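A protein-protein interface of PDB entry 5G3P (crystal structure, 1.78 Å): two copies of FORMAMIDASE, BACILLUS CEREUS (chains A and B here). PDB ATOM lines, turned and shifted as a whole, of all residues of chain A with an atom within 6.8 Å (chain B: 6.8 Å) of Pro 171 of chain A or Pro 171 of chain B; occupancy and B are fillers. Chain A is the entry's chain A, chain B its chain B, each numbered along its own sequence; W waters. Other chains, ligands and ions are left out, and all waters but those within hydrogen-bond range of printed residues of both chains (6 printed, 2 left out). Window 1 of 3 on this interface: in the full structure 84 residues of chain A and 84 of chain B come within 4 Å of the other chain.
The backbone NH of Phe 297 of chain A is in hydrogen-bond range of the side-chain carboxylate of Glu 176 of chain B (2.9 Å).
N of Phe 297 of chain B sits at hydrogen-bond distance from OE1 of Glu 176 of chain A (2.9 Å).
The side-chain carboxylate (OE2) of Glu 172 of chain A is in salt-bridge range of the guanidinium group (NE) of Arg 175 of chain B, 2.8 Å away.
NE of Arg 175 of chain A lies within salt-bridge range of OE2 of Glu 172 of chain B (2.8 Å).
The guanidinium group (NH1) of Arg 175 of chain A is in hydrogen-bond range of the side-chain amide oxygen (OD1) of Asn 210 of chain A (2.9 Å).
The guanidinium group (NH1) of Arg 175 of chain B sits at hydrogen-bond distance from the side-chain amide oxygen (OD1) of Asn 210 of chain B, 2.9 Å away.
The backbone carbonyl oxygen of Ser 205 of chain B sits close to the side-chain amide oxygen of Gln 209 of chain B.
NH1 of Arg 175 of chain B is in hydrogen-bond range of O of Gln 209 of chain B (3.0 Å).
The backbone carbonyl oxygen of Ser 205 of chain A lies close to the side-chain amide oxygen of Gln 209 of chain A, at 3.4 Å.
The guanidinium group of Arg 175 of chain A sits at hydrogen-bond distance from the backbone carbonyl oxygen of Gln 209 of chain A, 3.0 Å away.
CG of Gln 209 of chain B touches O of Met 169 of chain A (3.6 Å).
Phe 170 of chain A touches Arg 175 of chain B.
CE1 of Phe 170 of chain A touches N of Leu 278 of chain B (3.6 Å).
Pro 171 of chain A touches Arg 175 of chain B.
Arg 175 of chain A touches Phe 170 of chain B.
Ser 205 of chain B touches Ser 205 of chain A.
NE2 of Gln 209 of chain B touches OG of Ser 205 of chain A, at 3.9 Å.
O of Met 169 of chain B touches CG of Gln 209 of chain A (3.5 Å).
CG of Pro 171 of chain B touches OE1 of Gln 209 of chain A (3.5 Å).
Arg 175 of chain B touches Phe 297 of chain A.
Pro 171 of chain B touches just these residues of chain A: Pro 171 (3.3 Å), Arg 175 (3.6 Å) and Gln 209 (3.5 Å).
Printed residues of chain A within 4 Å of Met 169 of chain B: Gln 209 (3.5 Å).
Printed residues of chain B within 4 Å of Phe 297 of chain A: Glu 172, Arg 175 and Glu 176.
Of the printed residues of chain A, Arg 175 of chain B touches Phe 170 (3.8 Å), Pro 171 (3.5 Å), Glu 172 (2.8 Å) and Phe 297 (3.6 Å).
The nearest residue of chain A that does not touch Pro 171 of chain B is Phe 297 of chain A (5.4 Å).
The nearest printed residue of chain A that does not touch Phe 297 of chain B is Leu 278 of chain A (4.2 Å).
Of the 16 printed residues of chain A, 10 touch a printed residue of chain B.
Along chain B the printed residues that touch a printed residue of chain A span positions 169 to 297.
Phe 170 of chain A touches Arg 175 of chain B, and with the chains exchanged Arg 175 of chain A touches Phe 170 of chain B.
Pro 171 of chain A touches Arg 175 of chain B, and with the chains exchanged Arg 175 of chain A touches Pro 171 of chain B.
Arg 175 of chain A touches Phe 297 of chain B, and with the chains exchanged Phe 297 of chain A touches Arg 175 of chain B.
Ser 205 of chain B touches its own counterpart, Ser 205 of chain A.
16 positions are printed for both chains.
Of the 24 pairs that touch across the chains among the printed residues, 24 have their exchanged pair printed and touching as well.
Water W2 lies within hydrogen-bond range of OD1 of Asn 206 of chain B (2.7 Å), OE1 of Gln 209 of chain B (2.7 Å), OG of Ser 205 of chain B (2.8 Å) and NE2 of Gln 209 of chain A (2.9 Å).
Water W3 lies within hydrogen-bond range of OE1 of Gln 209 of chain A (2.7 Å), OD1 of Asn 206 of chain A (2.7 Å), OG of Ser 205 of chain A (2.7 Å) and NE2 of Gln 209 of chain B (2.9 Å).
Water W5 lies within hydrogen-bond range of O of Met 169 of chain A (2.7 Å), NH2 of Arg 175 of chain B (2.9 Å) and O of Gln 209 of chain B (2.9 Å).
Water W1 lies within hydrogen-bond range of O of Met 169 of chain B (2.8 Å), NH2 of Arg 175 of chain A (2.9 Å) and O of Gln 209 of chain A (2.9 Å).
Water W4 lies within hydrogen-bond range of OE2 of Glu 172 of chain B (2.8 Å), N of Glu 172 of chain A (3.3 Å) and O of Pro 171 of chain A (3.4 Å).
Water W6 lies within hydrogen-bond range of OE2 of Glu 172 of chain A (2.8 Å), N of Glu 172 of chain B (3.3 Å) and O of Pro 171 of chain B (3.4 Å).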
ATOM      1  N   ASP A 167      -1.320   1.026  12.003  1.00  0.00           N
ATOM      2  CA  ASP A 167      -0.598   1.193  13.276  1.00  0.00           C
ATOM      3  C   ASP A 167      -1.336   2.134  14.218  1.00  0.00           C
ATOM      4  O   ASP A 167      -1.378   1.907  15.433  1.00  0.00           O
ATOM      5  CB  ASP A 167       0.770   1.802  13.071  1.00  0.00           C
ATOM      6  CG  ASP A 167       1.816   0.829  12.530  1.00  0.00           C
ATOM      7  OD1 ASP A 167       1.720  -0.409  12.708  1.00  0.00           O
ATOM      8  OD2 ASP A 167       2.768   1.364  11.913  1.00  0.00           O
ATOM      9  N   GLY A 168      -1.859   3.227  13.666  1.00  0.00           N
ATOM     10  CA  GLY A 168      -2.481   4.251  14.506  1.00  0.00           C
ATOM     11  C   GLY A 168      -3.808   3.886  15.130  1.00  0.00           C
ATOM     12  O   GLY A 168      -4.351   4.675  15.884  1.00  0.00           O
ATOM     13  N   MET A 169      -4.335   2.688  14.810  1.00  0.00           N
ATOM     14  CA  MET A 169      -5.522   2.166  15.468  1.00  0.00           C
ATOM     15  C   MET A 169      -5.235   1.446  16.768  1.00  0.00           C
ATOM     16  O   MET A 169      -6.165   1.123  17.495  1.00  0.00           O
ATOM     17  CB  MET A 169      -6.289   1.233  14.531  1.00  0.00           C
ATOM     18  CG  MET A 169      -6.759   1.883  13.248  1.00  0.00           C
ATOM     19  SD  MET A 169      -7.749   3.357  13.470  1.00  0.00           S
ATOM     20  CE  MET A 169      -8.565   3.465  11.857  1.00  0.00           C
ATOM     21  N   PHE A 170      -3.954   1.191  17.019  1.00  0.00           N
ATOM     22  CA  PHE A 170      -3.489   0.551  18.214  1.00  0.00           C
ATOM     23  C   PHE A 170      -2.975   1.604  19.149  1.00  0.00           C
ATOM     24  O   PHE A 170      -1.971   2.226  18.860  1.00  0.00           O
ATOM     25  CB  PHE A 170      -2.370  -0.468  17.885  1.00  0.00           C
ATOM     26  CG  PHE A 170      -2.818  -1.539  16.952  1.00  0.00           C
ATOM     27  CD1 PHE A 170      -3.396  -2.704  17.448  1.00  0.00           C
ATOM     28  CD2 PHE A 170      -2.705  -1.379  15.584  1.00  0.00           C
ATOM     29  CE1 PHE A 170      -3.832  -3.682  16.583  1.00  0.00           C
ATOM     30  CE2 PHE A 170      -3.152  -2.351  14.714  1.00  0.00           C
ATOM     31  CZ  PHE A 170      -3.710  -3.522  15.213  1.00  0.00           C
ATOM     32  N   PRO A 171      -3.653   1.795  20.295  1.00  0.00           N
ATOM     33  CA  PRO A 171      -3.182   2.821  21.232  1.00  0.00           C
ATOM     34  C   PRO A 171      -1.789   2.497  21.772  1.00  0.00           C
ATOM     35  O   PRO A 171      -1.071   3.386  22.190  1.00  0.00           O
ATOM     36  CB  PRO A 171      -4.211   2.777  22.359  1.00  0.00           C
ATOM     37  CG  PRO A 171      -4.850   1.446  22.262  1.00  0.00           C
ATOM     38  CD  PRO A 171      -4.879   1.144  20.781  1.00  0.00           C
ATOM     39  N   GLU A 172      -1.403   1.233  21.694  1.00  0.00           N
ATOM     40  CA  GLU A 172      -0.057   0.790  22.071  1.00  0.00           C
ATOM     41  C   GLU A 172       1.045   1.443  21.221  1.00  0.00           C
ATOM     42  O   GLU A 172       2.162   1.654  21.706  1.00  0.00           O
ATOM     43  CB  GLU A 172       0.039  -0.726  21.995  1.00  0.00           C
ATOM     44  CG  GLU A 172      -0.861  -1.473  22.979  1.00  0.00           C
ATOM     45  CD  GLU A 172      -2.329  -1.636  22.555  1.00  0.00           C
ATOM     46  OE1 GLU A 172      -2.683  -1.291  21.393  1.00  0.00           O
ATOM     47  OE2 GLU A 172      -3.145  -2.149  23.373  1.00  0.00           O
ATOM     48  N   VAL A 173       0.745   1.723  19.954  1.00  0.00           N
ATOM     49  CA  VAL A 173       1.712   2.403  19.061  1.00  0.00           C
ATOM     50  C   VAL A 173       1.976   3.828  19.526  1.00  0.00           C
ATOM     51  O   VAL A 173       3.109   4.238  19.691  1.00  0.00           O
ATOM     52  CB  VAL A 173       1.249   2.340  17.590  1.00  0.00           C
ATOM     53  CG1 VAL A 173       1.990   3.334  16.711  1.00  0.00           C
ATOM     54  CG2 VAL A 173       1.423   0.931  17.067  1.00  0.00           C
ATOM     55  N   ALA A 174       0.918   4.601  19.722  1.00  0.00           N
ATOM     56  CA  ALA A 174       1.076   5.986  20.170  1.00  0.00           C
ATOM     57  C   ALA A 174       1.735   6.043  21.549  1.00  0.00           C
ATOM     58  O   ALA A 174       2.595   6.895  21.804  1.00  0.00           O
ATOM     59  CB  ALA A 174      -0.273   6.727  20.197  1.00  0.00           C
ATOM     60  N   ARG A 175       1.335   5.121  22.444  1.00  0.00           N
ATOM     61  CA  ARG A 175       1.921   5.058  23.769  1.00  0.00           C
ATOM     62  C   ARG A 175       3.424   4.792  23.715  1.00  0.00           C
ATOM     63  O   ARG A 175       4.205   5.446  24.399  1.00  0.00           O
ATOM     64  CB  ARG A 175       1.214   3.950  24.604  1.00  0.00           C
ATOM     65  CG  ARG A 175       1.785   3.774  25.987  1.00  0.00           C
ATOM     66  CD  ARG A 175       1.406   4.943  26.854  1.00  0.00           C
ATOM     67  NE  ARG A 175       0.072   4.745  27.456  1.00  0.00           N
ATOM     68  CZ  ARG A 175      -0.702   5.706  27.940  1.00  0.00           C
ATOM     69  NH1 ARG A 175      -0.356   6.993  27.798  1.00  0.00           N
ATOM     70  NH2 ARG A 175      -1.818   5.382  28.617  1.00  0.00           N
ATOM     71  N   GLU A 176       3.814   3.841  22.880  1.00  0.00           N
ATOM     72  CA  GLU A 176       5.204   3.516  22.699  1.00  0.00           C
ATOM     73  C   GLU A 176       6.013   4.707  22.180  1.00  0.00           C
ATOM     74  O   GLU A 176       7.137   4.948  22.641  1.00  0.00           O
ATOM     75  CB  GLU A 176       5.332   2.329  21.715  1.00  0.00           C
ATOM     76  CG  GLU A 176       6.769   1.894  21.418  1.00  0.00           C
ATOM     77  CD  GLU A 176       7.496   1.285  22.603  1.00  0.00           C
ATOM     78  OE1 GLU A 176       6.888   1.138  23.730  1.00  0.00           O
ATOM     79  OE2 GLU A 176       8.703   0.928  22.439  1.00  0.00           O
ATOM     80  N   SER A 205      -7.360  10.720  20.009  1.00  0.00           N
ATOM     81  CA  SER A 205      -7.105   9.961  21.231  1.00  0.00           C
ATOM     82  C   SER A 205      -5.613   9.652  21.389  1.00  0.00           C
ATOM     83  O   SER A 205      -5.088   9.687  22.522  1.00  0.00           O
ATOM     84  CB  SER A 205      -7.957   8.678  21.320  1.00  0.00           C
ATOM     85  OG  SER A 205      -7.666   7.777  20.251  1.00  0.00           O
ATOM     86  N   ASN A 206      -4.926   9.381  20.272  1.00  0.00           N
ATOM     87  CA  ASN A 206      -3.477   9.133  20.306  1.00  0.00           C
ATOM     88  C   ASN A 206      -2.711  10.343  20.859  1.00  0.00           C
ATOM     89  O   ASN A 206      -1.693  10.193  21.547  1.00  0.00           O
ATOM     90  CB  ASN A 206      -2.934   8.808  18.908  1.00  0.00           C
ATOM     91  CG  ASN A 206      -3.334   7.429  18.418  1.00  0.00           C
ATOM     92  OD1 ASN A 206      -3.743   6.553  19.203  1.00  0.00           O
ATOM     93  ND2 ASN A 206      -3.168   7.200  17.098  1.00  0.00           N
ATOM     94  N   GLN A 209      -4.077  10.970  25.003  1.00  0.00           N
ATOM     95  CA  GLN A 209      -3.636   9.944  25.934  1.00  0.00           C
ATOM     96  C   GLN A 209      -2.162  10.045  26.311  1.00  0.00           C
ATOM     97  O   GLN A 209      -1.781   9.615  27.403  1.00  0.00           O
ATOM     98  CB  GLN A 209      -3.930   8.549  25.391  1.00  0.00           C
ATOM     99  CG  GLN A 209      -5.390   8.210  25.396  1.00  0.00           C
ATOM    100  CD  GLN A 209      -5.741   7.027  24.525  1.00  0.00           C
ATOM    101  OE1 GLN A 209      -4.926   6.549  23.733  1.00  0.00           O
ATOM    102  NE2 GLN A 209      -6.972   6.561  24.648  1.00  0.00           N
ATOM    103  N   ASN A 210      -1.367  10.679  25.439  1.00  0.00           N
ATOM    104  CA  ASN A 210       0.078  10.763  25.558  1.00  0.00           C
ATOM    105  C   ASN A 210       0.657  12.173  25.680  1.00  0.00           C
ATOM    106  O   ASN A 210       1.879  12.332  25.687  1.00  0.00           O
ATOM    107  CB  ASN A 210       0.661  10.057  24.337  1.00  0.00           C
ATOM    108  CG  ASN A 210       0.299   8.603  24.325  1.00  0.00           C
ATOM    109  OD1 ASN A 210       0.712   7.861  25.222  1.00  0.00           O
ATOM    110  ND2 ASN A 210      -0.548   8.186  23.376  1.00  0.00           N
ATOM    111  N   LEU A 278       0.479   5.960  34.179  1.00  0.00           N
ATOM    112  CA  LEU A 278       0.249   4.575  33.734  1.00  0.00           C
ATOM    113  C   LEU A 278       1.014   3.577  34.558  1.00  0.00           C
ATOM    114  O   LEU A 278       0.468   2.552  34.953  1.00  0.00           O
ATOM    115  CB  LEU A 278       0.613   4.411  32.242  1.00  0.00           C
ATOM    116  CG  LEU A 278       0.564   2.993  31.687  1.00  0.00           C
ATOM    117  CD1 LEU A 278      -0.849   2.451  31.695  1.00  0.00           C
ATOM    118  CD2 LEU A 278       1.122   2.968  30.272  1.00  0.00           C
ATOM    119  N   PHE A 297      -3.205  -8.515  29.787  1.00  0.00           N
ATOM    120  CA  PHE A 297      -2.847  -8.437  28.354  1.00  0.00           C
ATOM    121  C   PHE A 297      -1.388  -7.960  28.169  1.00  0.00           C
ATOM    122  O   PHE A 297      -0.732  -8.337  27.191  1.00  0.00           O
ATOM    123  CB  PHE A 297      -3.852  -7.601  27.543  1.00  0.00           C
ATOM    124  CG  PHE A 297      -3.496  -6.148  27.385  1.00  0.00           C
ATOM    125  CD1 PHE A 297      -2.641  -5.731  26.356  1.00  0.00           C
ATOM    126  CD2 PHE A 297      -4.029  -5.186  28.226  1.00  0.00           C
ATOM    127  CE1 PHE A 297      -2.290  -4.393  26.208  1.00  0.00           C
ATOM    128  CE2 PHE A 297      -3.689  -3.843  28.065  1.00  0.00           C
ATOM    129  CZ  PHE A 297      -2.822  -3.454  27.060  1.00  0.00           C
ATOM    130  N   ASP B 167      -9.629   6.020  35.049  1.00  0.00           N
ATOM    131  CA  ASP B 167      -9.270   4.733  34.418  1.00  0.00           C
ATOM    132  C   ASP B 167      -9.517   4.740  32.923  1.00  0.00           C
ATOM    133  O   ASP B 167      -8.718   4.225  32.139  1.00  0.00           O
ATOM    134  CB  ASP B 167     -10.124   3.565  34.955  1.00  0.00           C
ATOM    135  CG  ASP B 167      -9.734   3.084  36.332  1.00  0.00           C
ATOM    136  OD1 ASP B 167      -8.567   3.188  36.762  1.00  0.00           O
ATOM    137  OD2 ASP B 167     -10.658   2.518  36.976  1.00  0.00           O
ATOM    138  N   GLY B 168     -10.618   5.369  32.512  1.00  0.00           N
ATOM    139  CA  GLY B 168     -10.984   5.401  31.116  1.00  0.00           C
ATOM    140  C   GLY B 168     -10.138   6.271  30.204  1.00  0.00           C
ATOM    141  O   GLY B 168     -10.352   6.253  28.990  1.00  0.00           O
ATOM    142  N   MET B 169      -9.193   7.031  30.770  1.00  0.00           N
ATOM    143  CA  MET B 169      -8.218   7.769  29.979  1.00  0.00           C
ATOM    144  C   MET B 169      -6.997   6.943  29.560  1.00  0.00           C
ATOM    145  O   MET B 169      -6.205   7.398  28.740  1.00  0.00           O
ATOM    146  CB  MET B 169      -7.711   9.000  30.758  1.00  0.00           C
ATOM    147  CG  MET B 169      -8.798   9.983  31.128  1.00  0.00           C
ATOM    148  SD  MET B 169      -9.787  10.536  29.754  1.00  0.00           S
ATOM    149  CE  MET B 169     -10.523  12.028  30.461  1.00  0.00           C
ATOM    150  N   PHE B 170      -6.885   5.739  30.122  1.00  0.00           N
ATOM    151  CA  PHE B 170      -5.833   4.796  29.807  1.00  0.00           C
ATOM    152  C   PHE B 170      -6.392   3.783  28.852  1.00  0.00           C
ATOM    153  O   PHE B 170      -7.245   2.984  29.227  1.00  0.00           O
ATOM    154  CB  PHE B 170      -5.321   4.107  31.074  1.00  0.00           C
ATOM    155  CG  PHE B 170      -4.765   5.066  32.059  1.00  0.00           C
ATOM    156  CD1 PHE B 170      -3.426   5.438  32.007  1.00  0.00           C
ATOM    157  CD2 PHE B 170      -5.598   5.644  33.002  1.00  0.00           C
ATOM    158  CE1 PHE B 170      -2.937   6.370  32.896  1.00  0.00           C
ATOM    159  CE2 PHE B 170      -5.102   6.572  33.912  1.00  0.00           C
ATOM    160  CZ  PHE B 170      -3.766   6.927  33.861  1.00  0.00           C
ATOM    161  N   PRO B 171      -5.894   3.782  27.614  1.00  0.00           N
ATOM    162  CA  PRO B 171      -6.384   2.757  26.666  1.00  0.00           C
ATOM    163  C   PRO B 171      -6.112   1.339  27.121  1.00  0.00           C
ATOM    164  O   PRO B 171      -6.794   0.412  26.690  1.00  0.00           O
ATOM    165  CB  PRO B 171      -5.624   3.076  25.363  1.00  0.00           C
ATOM    166  CG  PRO B 171      -4.429   3.839  25.815  1.00  0.00           C
ATOM    167  CD  PRO B 171      -4.900   4.653  27.000  1.00  0.00           C
ATOM    168  N   GLU B 172      -5.139   1.174  27.997  1.00  0.00           N
ATOM    169  CA  GLU B 172      -4.818  -0.122  28.577  1.00  0.00           C
ATOM    170  C   GLU B 172      -5.958  -0.699  29.376  1.00  0.00           C
ATOM    171  O   GLU B 172      -6.108  -1.933  29.460  1.00  0.00           O
ATOM    172  CB  GLU B 172      -3.541  -0.016  29.428  1.00  0.00           C
ATOM    173  CG  GLU B 172      -2.247   0.326  28.673  1.00  0.00           C
ATOM    174  CD  GLU B 172      -2.074   1.830  28.358  1.00  0.00           C
ATOM    175  OE1 GLU B 172      -2.884   2.678  28.826  1.00  0.00           O
ATOM    176  OE2 GLU B 172      -1.108   2.180  27.645  1.00  0.00           O
ATOM    177  N   VAL B 173      -6.755   0.160  30.007  1.00  0.00           N
ATOM    178  CA  VAL B 173      -7.912  -0.301  30.782  1.00  0.00           C
ATOM    179  C   VAL B 173      -8.988  -0.911  29.847  1.00  0.00           C
ATOM    180  O   VAL B 173      -9.452  -2.016  30.075  1.00  0.00           O
ATOM    181  CB  VAL B 173      -8.508   0.846  31.637  1.00  0.00           C
ATOM    182  CG1 VAL B 173      -9.911   0.530  32.134  1.00  0.00           C
ATOM    183  CG2 VAL B 173      -7.586   1.111  32.797  1.00  0.00           C
ATOM    184  N   ALA B 174      -9.372  -0.187  28.813  1.00  0.00           N
ATOM    185  CA  ALA B 174     -10.364  -0.702  27.856  1.00  0.00           C
ATOM    186  C   ALA B 174      -9.848  -1.965  27.157  1.00  0.00           C
ATOM    187  O   ALA B 174     -10.618  -2.925  26.964  1.00  0.00           O
ATOM    188  CB  ALA B 174     -10.739   0.352  26.838  1.00  0.00           C
ATOM    189  N   ARG B 175      -8.565  -1.974  26.806  1.00  0.00           N
ATOM    190  CA  ARG B 175      -7.960  -3.131  26.153  1.00  0.00           C
ATOM    191  C   ARG B 175      -8.043  -4.355  27.054  1.00  0.00           C
ATOM    192  O   ARG B 175      -8.407  -5.438  26.610  1.00  0.00           O
ATOM    193  CB  ARG B 175      -6.517  -2.822  25.765  1.00  0.00           C
ATOM    194  CG  ARG B 175      -5.786  -3.980  25.145  1.00  0.00           C
ATOM    195  CD  ARG B 175      -6.302  -4.204  23.748  1.00  0.00           C
ATOM    196  NE  ARG B 175      -5.624  -3.331  22.767  1.00  0.00           N
ATOM    197  CZ  ARG B 175      -6.090  -3.025  21.563  1.00  0.00           C
ATOM    198  NH1 ARG B 175      -7.314  -3.381  21.195  1.00  0.00           N
ATOM    199  NH2 ARG B 175      -5.304  -2.345  20.713  1.00  0.00           N
ATOM    200  N   GLU B 176      -7.662  -4.177  28.320  1.00  0.00           N
ATOM    201  CA  GLU B 176      -7.734  -5.240  29.301  1.00  0.00           C
ATOM    202  C   GLU B 176      -9.139  -5.798  29.474  1.00  0.00           C
ATOM    203  O   GLU B 176      -9.324  -7.029  29.534  1.00  0.00           O
ATOM    204  CB  GLU B 176      -7.205  -4.744  30.656  1.00  0.00           C
ATOM    205  CG  GLU B 176      -7.223  -5.785  31.769  1.00  0.00           C
ATOM    206  CD  GLU B 176      -6.242  -6.920  31.565  1.00  0.00           C
ATOM    207  OE1 GLU B 176      -5.491  -6.946  30.525  1.00  0.00           O
ATOM    208  OE2 GLU B 176      -6.225  -7.837  32.454  1.00  0.00           O
ATOM    209  N   SER B 205     -13.054   6.095  21.589  1.00  0.00           N
ATOM    210  CA  SER B 205     -11.838   5.355  21.191  1.00  0.00           C
ATOM    211  C   SER B 205     -11.742   4.018  21.948  1.00  0.00           C
ATOM    212  O   SER B 205     -11.338   3.013  21.366  1.00  0.00           O
ATOM    213  CB  SER B 205     -10.563   6.189  21.355  1.00  0.00           C
ATOM    214  OG  SER B 205     -10.352   6.573  22.698  1.00  0.00           O
ATOM    215  N   ASN B 206     -12.165   4.009  23.218  1.00  0.00           N
ATOM    216  CA  ASN B 206     -12.218   2.802  23.990  1.00  0.00           C
ATOM    217  C   ASN B 206     -13.123   1.736  23.342  1.00  0.00           C
ATOM    218  O   ASN B 206     -12.835   0.538  23.443  1.00  0.00           O
ATOM    219  CB  ASN B 206     -12.709   3.069  25.418  1.00  0.00           C
ATOM    220  CG  ASN B 206     -11.669   3.782  26.294  1.00  0.00           C
ATOM    221  OD1 ASN B 206     -10.479   3.857  25.969  1.00  0.00           O
ATOM    222  ND2 ASN B 206     -12.140   4.307  27.431  1.00  0.00           N
ATOM    223  N   GLN B 209     -11.438   0.763  19.445  1.00  0.00           N
ATOM    224  CA  GLN B 209     -10.165   0.031  19.474  1.00  0.00           C
ATOM    225  C   GLN B 209     -10.336  -1.429  19.847  1.00  0.00           C
ATOM    226  O   GLN B 209      -9.501  -2.250  19.462  1.00  0.00           O
ATOM    227  CB  GLN B 209      -9.177   0.701  20.427  1.00  0.00           C
ATOM    228  CG  GLN B 209      -8.640   2.003  19.895  1.00  0.00           C
ATOM    229  CD  GLN B 209      -7.981   2.864  20.939  1.00  0.00           C
ATOM    230  OE1 GLN B 209      -8.087   2.610  22.138  1.00  0.00           O
ATOM    231  NE2 GLN B 209      -7.328   3.919  20.495  1.00  0.00           N
ATOM    232  N   ASN B 210     -11.441  -1.735  20.533  1.00  0.00           N
ATOM    233  CA  ASN B 210     -11.715  -3.042  21.087  1.00  0.00           C
ATOM    234  C   ASN B 210     -12.956  -3.762  20.578  1.00  0.00           C
ATOM    235  O   ASN B 210     -13.295  -4.826  21.105  1.00  0.00           O
ATOM    236  CB  ASN B 210     -11.792  -2.854  22.616  1.00  0.00           C
ATOM    237  CG  ASN B 210     -10.472  -2.386  23.180  1.00  0.00           C
ATOM    238  OD1 ASN B 210      -9.480  -3.113  23.108  1.00  0.00           O
ATOM    239  ND2 ASN B 210     -10.432  -1.173  23.708  1.00  0.00           N
ATOM    240  N   LEU B 278      -3.487  -7.185  17.481  1.00  0.00           N
ATOM    241  CA  LEU B 278      -2.490  -6.600  18.378  1.00  0.00           C
ATOM    242  C   LEU B 278      -1.352  -7.570  18.652  1.00  0.00           C
ATOM    243  O   LEU B 278      -0.185  -7.184  18.642  1.00  0.00           O
ATOM    244  CB  LEU B 278      -3.122  -6.174  19.711  1.00  0.00           C
ATOM    245  CG  LEU B 278      -2.164  -5.702  20.818  1.00  0.00           C
ATOM    246  CD1 LEU B 278      -1.446  -4.419  20.403  1.00  0.00           C
ATOM    247  CD2 LEU B 278      -2.920  -5.470  22.115  1.00  0.00           C
ATOM    248  N   PHE B 297       7.450  -0.277  26.159  1.00  0.00           N
ATOM    249  CA  PHE B 297       6.656   0.117  27.326  1.00  0.00           C
ATOM    250  C   PHE B 297       5.912  -1.098  27.923  1.00  0.00           C
ATOM    251  O   PHE B 297       5.663  -1.161  29.137  1.00  0.00           O
ATOM    252  CB  PHE B 297       5.692   1.297  27.024  1.00  0.00           C
ATOM    253  CG  PHE B 297       4.299   0.892  26.587  1.00  0.00           C
ATOM    254  CD1 PHE B 297       3.309   0.606  27.539  1.00  0.00           C
ATOM    255  CD2 PHE B 297       3.970   0.827  25.236  1.00  0.00           C
ATOM    256  CE1 PHE B 297       2.026   0.261  27.152  1.00  0.00           C
ATOM    257  CE2 PHE B 297       2.667   0.496  24.838  1.00  0.00           C
ATOM    258  CZ  PHE B 297       1.711   0.191  25.791  1.00  0.00           C
HETATM  259  O   HOH W   1      -3.465   7.722  28.760  1.00  0.00           O
HETATM  260  O   HOH W   2      -8.886   4.482  23.905  1.00  0.00           O
HETATM  261  O   HOH W   3      -5.619   6.193  21.160  1.00  0.00           O
HETATM  262  O   HOH W   4      -1.539   1.551  24.993  1.00  0.00           O
HETATM  263  O   HOH W   5      -6.897  -1.247  18.541  1.00  0.00           O
HETATM  264  O   HOH W   6      -3.748  -0.309  25.365  1.00  0.00           O
